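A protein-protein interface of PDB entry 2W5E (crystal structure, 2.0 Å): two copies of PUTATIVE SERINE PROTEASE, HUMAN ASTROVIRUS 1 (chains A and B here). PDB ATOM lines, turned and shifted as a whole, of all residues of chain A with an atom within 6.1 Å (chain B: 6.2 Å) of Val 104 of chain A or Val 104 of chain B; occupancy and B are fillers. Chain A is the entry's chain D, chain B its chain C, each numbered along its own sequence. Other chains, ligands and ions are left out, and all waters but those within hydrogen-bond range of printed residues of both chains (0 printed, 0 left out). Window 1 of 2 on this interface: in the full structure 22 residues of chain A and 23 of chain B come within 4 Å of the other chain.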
ATOM      1  N   ILE A   8      32.159 -16.299  -1.558  1.00  0.00           N
ATOM      2  CA  ILE A   8      31.873 -14.879  -1.417  1.00  0.00           C
ATOM      3  C   ILE A   8      33.149 -14.159  -0.989  1.00  0.00           C
ATOM      4  O   ILE A   8      33.723 -14.455   0.061  1.00  0.00           O
ATOM      5  CB  ILE A   8      30.711 -14.624  -0.432  1.00  0.00           C
ATOM      6  CG1 ILE A   8      29.438 -15.320  -0.938  1.00  0.00           C
ATOM      7  CG2 ILE A   8      30.470 -13.122  -0.243  1.00  0.00           C
ATOM      8  CD1 ILE A   8      28.350 -15.443   0.097  1.00  0.00           C
ATOM      9  N   PRO A  10      34.618 -10.578  -0.295  1.00  0.00           N
ATOM     10  CA  PRO A  10      34.543  -9.146   0.001  1.00  0.00           C
ATOM     11  C   PRO A  10      35.879  -8.435  -0.206  1.00  0.00           C
ATOM     12  O   PRO A  10      35.896  -7.229  -0.456  1.00  0.00           O
ATOM     13  CB  PRO A  10      34.163  -9.118   1.484  1.00  0.00           C
ATOM     14  CG  PRO A  10      33.542 -10.470   1.733  1.00  0.00           C
ATOM     15  CD  PRO A  10      34.395 -11.374   0.922  1.00  0.00           C
ATOM     16  N   THR A  93      24.248 -13.384  -5.480  1.00  0.00           N
ATOM     17  CA  THR A  93      24.828 -12.773  -4.288  1.00  0.00           C
ATOM     18  C   THR A  93      25.290 -11.388  -4.725  1.00  0.00           C
ATOM     19  O   THR A  93      26.036 -11.262  -5.699  1.00  0.00           O
ATOM     20  CB  THR A  93      26.032 -13.581  -3.720  1.00  0.00           C
ATOM     21  OG1 THR A  93      25.598 -14.887  -3.311  1.00  0.00           O
ATOM     22  CG2 THR A  93      26.630 -12.870  -2.501  1.00  0.00           C
ATOM     23  N   VAL A  94      24.801 -10.354  -4.042  1.00  0.00           N
ATOM     24  CA  VAL A  94      25.217  -8.977  -4.335  1.00  0.00           C
ATOM     25  C   VAL A  94      26.099  -8.487  -3.195  1.00  0.00           C
ATOM     26  O   VAL A  94      25.736  -8.614  -2.025  1.00  0.00           O
ATOM     27  CB  VAL A  94      24.016  -8.009  -4.555  1.00  0.00           C
ATOM     28  CG1 VAL A  94      24.511  -6.620  -5.002  1.00  0.00           C
ATOM     29  CG2 VAL A  94      23.037  -8.575  -5.589  1.00  0.00           C
ATOM     30  N   MET A  95      27.265  -7.955  -3.548  1.00  0.00           N
ATOM     31  CA  MET A  95      28.246  -7.460  -2.581  1.00  0.00           C
ATOM     32  C   MET A  95      28.517  -5.995  -2.866  1.00  0.00           C
ATOM     33  O   MET A  95      28.833  -5.646  -4.000  1.00  0.00           O
ATOM     34  CB  MET A  95      29.575  -8.200  -2.735  1.00  0.00           C
ATOM     35  CG  MET A  95      29.590  -9.632  -2.287  1.00  0.00           C
ATOM     36  SD  MET A  95      31.273 -10.286  -2.352  1.00  0.00           S
ATOM     37  CE  MET A  95      31.733 -10.043  -4.075  1.00  0.00           C
ATOM     38  N   ALA A  96      28.421  -5.143  -1.845  1.00  0.00           N
ATOM     39  CA  ALA A  96      28.622  -3.704  -2.048  1.00  0.00           C
ATOM     40  C   ALA A  96      29.148  -2.984  -0.823  1.00  0.00           C
ATOM     41  O   ALA A  96      28.925  -3.424   0.310  1.00  0.00           O
ATOM     42  CB  ALA A  96      27.316  -3.037  -2.517  1.00  0.00           C
ATOM     43  N   LEU A 102      30.322  -2.726   4.453  1.00  0.00           N
ATOM     44  CA  LEU A 102      30.090  -3.816   3.529  1.00  0.00           C
ATOM     45  C   LEU A 102      28.651  -4.301   3.707  1.00  0.00           C
ATOM     46  O   LEU A 102      28.177  -4.460   4.830  1.00  0.00           O
ATOM     47  CB  LEU A 102      31.061  -4.977   3.795  1.00  0.00           C
ATOM     48  CG  LEU A 102      30.767  -6.290   3.043  1.00  0.00           C
ATOM     49  CD1 LEU A 102      31.071  -6.135   1.569  1.00  0.00           C
ATOM     50  CD2 LEU A 102      31.526  -7.479   3.627  1.00  0.00           C
ATOM     51  N   VAL A 103      27.963  -4.518   2.596  1.00  0.00           N
ATOM     52  CA  VAL A 103      26.637  -5.127   2.614  1.00  0.00           C
ATOM     53  C   VAL A 103      26.649  -6.288   1.622  1.00  0.00           C
ATOM     54  O   VAL A 103      27.008  -6.113   0.462  1.00  0.00           O
ATOM     55  CB  VAL A 103      25.515  -4.100   2.281  1.00  0.00           C
ATOM     56  CG1 VAL A 103      24.157  -4.788   2.147  1.00  0.00           C
ATOM     57  CG2 VAL A 103      25.430  -3.039   3.366  1.00  0.00           C
ATOM     58  N   VAL A 104      26.306  -7.480   2.105  1.00  0.00           N
ATOM     59  CA  VAL A 104      26.168  -8.664   1.251  1.00  0.00           C
ATOM     60  C   VAL A 104      24.781  -9.254   1.475  1.00  0.00           C
ATOM     61  O   VAL A 104      24.345  -9.390   2.616  1.00  0.00           O
ATOM     62  CB  VAL A 104      27.216  -9.767   1.576  1.00  0.00           C
ATOM     63  CG1 VAL A 104      27.150 -10.897   0.538  1.00  0.00           C
ATOM     64  CG2 VAL A 104      28.642  -9.185   1.667  1.00  0.00           C
ATOM     65  N   SER A 105      24.092  -9.592   0.389  1.00  0.00           N
ATOM     66  CA  SER A 105      22.810 -10.294   0.487  1.00  0.00           C
ATOM     67  C   SER A 105      22.536 -11.161  -0.738  1.00  0.00           C
ATOM     68  O   SER A 105      23.044 -10.894  -1.825  1.00  0.00           O
ATOM     69  CB  SER A 105      21.660  -9.307   0.684  1.00  0.00           C
ATOM     70  OG  SER A 105      21.563  -8.442  -0.432  1.00  0.00           O
ATOM     71  N   THR A 106      21.733 -12.203  -0.553  1.00  0.00           N
ATOM     72  CA  THR A 106      21.297 -13.022  -1.675  1.00  0.00           C
ATOM     73  C   THR A 106      19.893 -12.599  -2.109  1.00  0.00           C
ATOM     74  O   THR A 106      19.178 -11.924  -1.359  1.00  0.00           O
ATOM     75  CB  THR A 106      21.290 -14.523  -1.316  1.00  0.00           C
ATOM     76  OG1 THR A 106      20.407 -14.743  -0.210  1.00  0.00           O
ATOM     77  CG2 THR A 106      22.707 -15.000  -0.948  1.00  0.00           C
ATOM     78  N   ARG A 121      18.345  -5.322  -0.284  1.00  0.00           N
ATOM     79  CA  ARG A 121      18.021  -5.125   1.133  1.00  0.00           C
ATOM     80  C   ARG A 121      17.925  -3.649   1.513  1.00  0.00           C
ATOM     81  O   ARG A 121      17.163  -3.278   2.410  1.00  0.00           O
ATOM     82  CB  ARG A 121      19.040  -5.846   2.025  1.00  0.00           C
ATOM     83  CG  ARG A 121      18.932  -7.373   1.986  1.00  0.00           C
ATOM     84  CD  ARG A 121      17.884  -7.889   2.958  1.00  0.00           C
ATOM     85  NE  ARG A 121      17.286  -9.152   2.520  1.00  0.00           N
ATOM     86  CZ  ARG A 121      16.354  -9.816   3.201  1.00  0.00           C
ATOM     87  NH1 ARG A 121      15.905  -9.344   4.360  1.00  0.00           N
ATOM     88  NH2 ARG A 121      15.864 -10.953   2.726  1.00  0.00           N
ATOM     89  N   ILE B   8      35.045 -14.115   6.216  1.00  0.00           N
ATOM     90  CA  ILE B   8      33.597 -14.215   6.376  1.00  0.00           C
ATOM     91  C   ILE B   8      33.134 -15.571   5.837  1.00  0.00           C
ATOM     92  O   ILE B   8      33.349 -15.889   4.666  1.00  0.00           O
ATOM     93  CB  ILE B   8      32.874 -13.035   5.671  1.00  0.00           C
ATOM     94  CG1 ILE B   8      33.281 -11.707   6.326  1.00  0.00           C
ATOM     95  CG2 ILE B   8      31.354 -13.221   5.707  1.00  0.00           C
ATOM     96  CD1 ILE B   8      32.931 -10.462   5.523  1.00  0.00           C
ATOM     97  N   PRO B  10      29.917 -17.865   5.429  1.00  0.00           N
ATOM     98  CA  PRO B  10      28.484 -18.212   5.413  1.00  0.00           C
ATOM     99  C   PRO B  10      28.214 -19.714   5.546  1.00  0.00           C
ATOM    100  O   PRO B  10      27.104 -20.107   5.913  1.00  0.00           O
ATOM    101  CB  PRO B  10      28.018 -17.711   4.041  1.00  0.00           C
ATOM    102  CG  PRO B  10      29.025 -16.648   3.667  1.00  0.00           C
ATOM    103  CD  PRO B  10      30.323 -17.180   4.187  1.00  0.00           C
ATOM    104  N   THR B  93      31.419  -7.940  12.055  1.00  0.00           N
ATOM    105  CA  THR B  93      30.719  -8.480  10.895  1.00  0.00           C
ATOM    106  C   THR B  93      29.586  -9.350  11.439  1.00  0.00           C
ATOM    107  O   THR B  93      29.827 -10.240  12.253  1.00  0.00           O
ATOM    108  CB  THR B  93      31.653  -9.352  10.021  1.00  0.00           C
ATOM    109  OG1 THR B  93      32.741  -8.560   9.527  1.00  0.00           O
ATOM    110  CG2 THR B  93      30.897  -9.944   8.833  1.00  0.00           C
ATOM    111  N   VAL B  94      28.354  -9.078  11.007  1.00  0.00           N
ATOM    112  CA  VAL B  94      27.198  -9.898  11.399  1.00  0.00           C
ATOM    113  C   VAL B  94      26.713 -10.671  10.177  1.00  0.00           C
ATOM    114  O   VAL B  94      26.514 -10.077   9.124  1.00  0.00           O
ATOM    115  CB  VAL B  94      26.014  -9.035  11.936  1.00  0.00           C
ATOM    116  CG1 VAL B  94      24.906  -9.931  12.501  1.00  0.00           C
ATOM    117  CG2 VAL B  94      26.480  -8.033  12.990  1.00  0.00           C
ATOM    118  N   MET B  95      26.535 -11.987  10.320  1.00  0.00           N
ATOM    119  CA  MET B  95      25.976 -12.823   9.240  1.00  0.00           C
ATOM    120  C   MET B  95      24.744 -13.521   9.754  1.00  0.00           C
ATOM    121  O   MET B  95      24.771 -14.082  10.843  1.00  0.00           O
ATOM    122  CB  MET B  95      26.921 -13.943   8.792  1.00  0.00           C
ATOM    123  CG  MET B  95      28.402 -13.715   8.840  1.00  0.00           C
ATOM    124  SD  MET B  95      29.182 -15.229   8.220  1.00  0.00           S
ATOM    125  CE  MET B  95      29.305 -16.237   9.698  1.00  0.00           C
ATOM    126  N   ALA B  96      23.679 -13.537   8.958  1.00  0.00           N
ATOM    127  CA  ALA B  96      22.451 -14.221   9.360  1.00  0.00           C
ATOM    128  C   ALA B  96      21.647 -14.728   8.175  1.00  0.00           C
ATOM    129  O   ALA B  96      21.846 -14.293   7.041  1.00  0.00           O
ATOM    130  CB  ALA B  96      21.582 -13.292  10.221  1.00  0.00           C
ATOM    131  N   LEU B 102      20.643 -15.062   2.789  1.00  0.00           N
ATOM    132  CA  LEU B 102      21.837 -14.741   3.568  1.00  0.00           C
ATOM    133  C   LEU B 102      21.976 -13.226   3.592  1.00  0.00           C
ATOM    134  O   LEU B 102      21.766 -12.572   2.573  1.00  0.00           O
ATOM    135  CB  LEU B 102      23.092 -15.358   2.931  1.00  0.00           C
ATOM    136  CG  LEU B 102      24.446 -14.843   3.458  1.00  0.00           C
ATOM    137  CD1 LEU B 102      24.717 -15.330   4.872  1.00  0.00           C
ATOM    138  CD2 LEU B 102      25.584 -15.222   2.519  1.00  0.00           C
ATOM    139  N   VAL B 103      22.296 -12.674   4.762  1.00  0.00           N
ATOM    140  CA  VAL B 103      22.541 -11.239   4.917  1.00  0.00           C
ATOM    141  C   VAL B 103      23.825 -11.044   5.730  1.00  0.00           C
ATOM    142  O   VAL B 103      23.955 -11.578   6.832  1.00  0.00           O
ATOM    143  CB  VAL B 103      21.340 -10.505   5.601  1.00  0.00           C
ATOM    144  CG1 VAL B 103      21.676  -9.046   5.888  1.00  0.00           C
ATOM    145  CG2 VAL B 103      20.083 -10.578   4.728  1.00  0.00           C
ATOM    146  N   VAL B 104      24.770 -10.294   5.167  1.00  0.00           N
ATOM    147  CA  VAL B 104      26.028  -9.969   5.850  1.00  0.00           C
ATOM    148  C   VAL B 104      26.192  -8.456   5.871  1.00  0.00           C
ATOM    149  O   VAL B 104      25.997  -7.798   4.848  1.00  0.00           O
ATOM    150  CB  VAL B 104      27.272 -10.586   5.139  1.00  0.00           C
ATOM    151  CG1 VAL B 104      28.560 -10.306   5.934  1.00  0.00           C
ATOM    152  CG2 VAL B 104      27.098 -12.090   4.899  1.00  0.00           C
ATOM    153  N   SER B 105      26.541  -7.911   7.036  1.00  0.00           N
ATOM    154  CA  SER B 105      26.884  -6.491   7.141  1.00  0.00           C
ATOM    155  C   SER B 105      27.977  -6.210   8.175  1.00  0.00           C
ATOM    156  O   SER B 105      28.143  -6.950   9.154  1.00  0.00           O
ATOM    157  CB  SER B 105      25.639  -5.632   7.417  1.00  0.00           C
ATOM    158  OG  SER B 105      25.054  -5.958   8.664  1.00  0.00           O
ATOM    159  N   THR B 106      28.719  -5.132   7.940  1.00  0.00           N
ATOM    160  CA  THR B 106      29.680  -4.615   8.913  1.00  0.00           C
ATOM    161  C   THR B 106      29.069  -3.444   9.688  1.00  0.00           C
ATOM    162  O   THR B 106      28.075  -2.854   9.251  1.00  0.00           O
ATOM    163  CB  THR B 106      30.985  -4.160   8.229  1.00  0.00           C
ATOM    164  OG1 THR B 106      30.684  -3.175   7.238  1.00  0.00           O
ATOM    165  CG2 THR B 106      31.685  -5.341   7.554  1.00  0.00           C
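CD1 of Ile 8 of chain A touches CG of Pro 10 of chain B, at 3.8 Å. Ile 8 of chain A touches Leu 102 of chain B. Ile 8 of chain B touches Pro 10 of chain A. Ile 8 of chain B touches Leu 102 of chain A. O of Val 104 of chain B touches O of Leu 102 of chain A, at 3.99 Å. Leu 102 of chain A touches Ser 105 of chain B. Val 103 of chain A touches Val 104 of chain B. CA of Val 103 of chain B touches O of Val 104 of chain A, at 3.5 Å. O of Leu 102 of chain B touches CA of Ser 105 of chain A, 3.3 Å away. CG2 of Val 103 of chain B touches NE of Arg 121 of chain A, at 3.8 Å.
N of Val 94 of chain B lies within hydrogen-bond range of O of Ser 105 of chain B (2.8 Å). The backbone carbonyl oxygen of Ala 96 of chain B is in hydrogen-bond range of the backbone NH of Val 103 of chain B, at 2.8 Å. The backbone NH (N) of Val 94 of chain A is in hydrogen-bond range of the backbone carbonyl oxygen (O) of Ser 105 of chain A, 2.9 Å away. The backbone carbonyl oxygen of Ala 96 of chain A is in hydrogen-bond range of the backbone NH of Val 103 of chain A, 2.7 Å away.
OG1 of Thr 106 of chain A lies within hydrogen-bond range of N of Leu 102 of chain B (3.0 Å). The backbone NH of Val 104 of chain B sits at hydrogen-bond distance from the backbone carbonyl oxygen of Val 104 of chain A. N of Leu 102 of chain A sits at hydrogen-bond distance from OG1 of Thr 106 of chain B, 2.8 Å away.
Ile 8 of chain A touches Pro 10 of chain B, and with the chains exchanged Pro 10 of chain A touches Ile 8 of chain B. Ile 8 of chain A touches Leu 102 of chain B, and with the chains exchanged Leu 102 of chain A touches Ile 8 of chain B. Leu 102 of chain A touches Val 104 of chain B, but with the chains exchanged Val 104 of chain A does not touch Leu 102 of chain B (4.1 Å). Leu 102 of chain A touches Ser 105 of chain B, and with the chains exchanged Ser 105 of chain A touches Leu 102 of chain B. Of the 13 pairs that touch across the chains among the printed residues, 11 have their exchanged pair printed and touching as well.
Printed residues of chain A within 4 Å of Val 104 of chain B: Leu 102 (3.99 Å), Val 103 (3.5 Å) and Val 104 (2.7 Å). Printed residues of chain A within 4 Å of Val 103 of chain B: Val 104 and Arg 121. Of the printed residues of chain B, Arg 121 of chain A touches Val 103. The nearest printed residue of chain A that does not touch Val 104 of chain B is Ser 105 of chain A (4.9 Å). The nearest printed residue of chain B that does not touch Ile 8 of chain A is Ile 8 of chain B (4.8 Å).
Along chain A the printed residues that touch a printed residue of chain B span positions 8 to 121. Of the 11 printed residues of chain B, 7 touch a printed residue of chain A. Printed residues of chain B that touch a printed residue of chain A: Ile 8, Pro 10, Leu 102, Val 103, Val 104, Ser 105 and Thr 106. Among the printed residues, no Asp or Glu carboxylate lies within 4 Å of a Lys or Arg side-chain nitrogen of the other chain.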
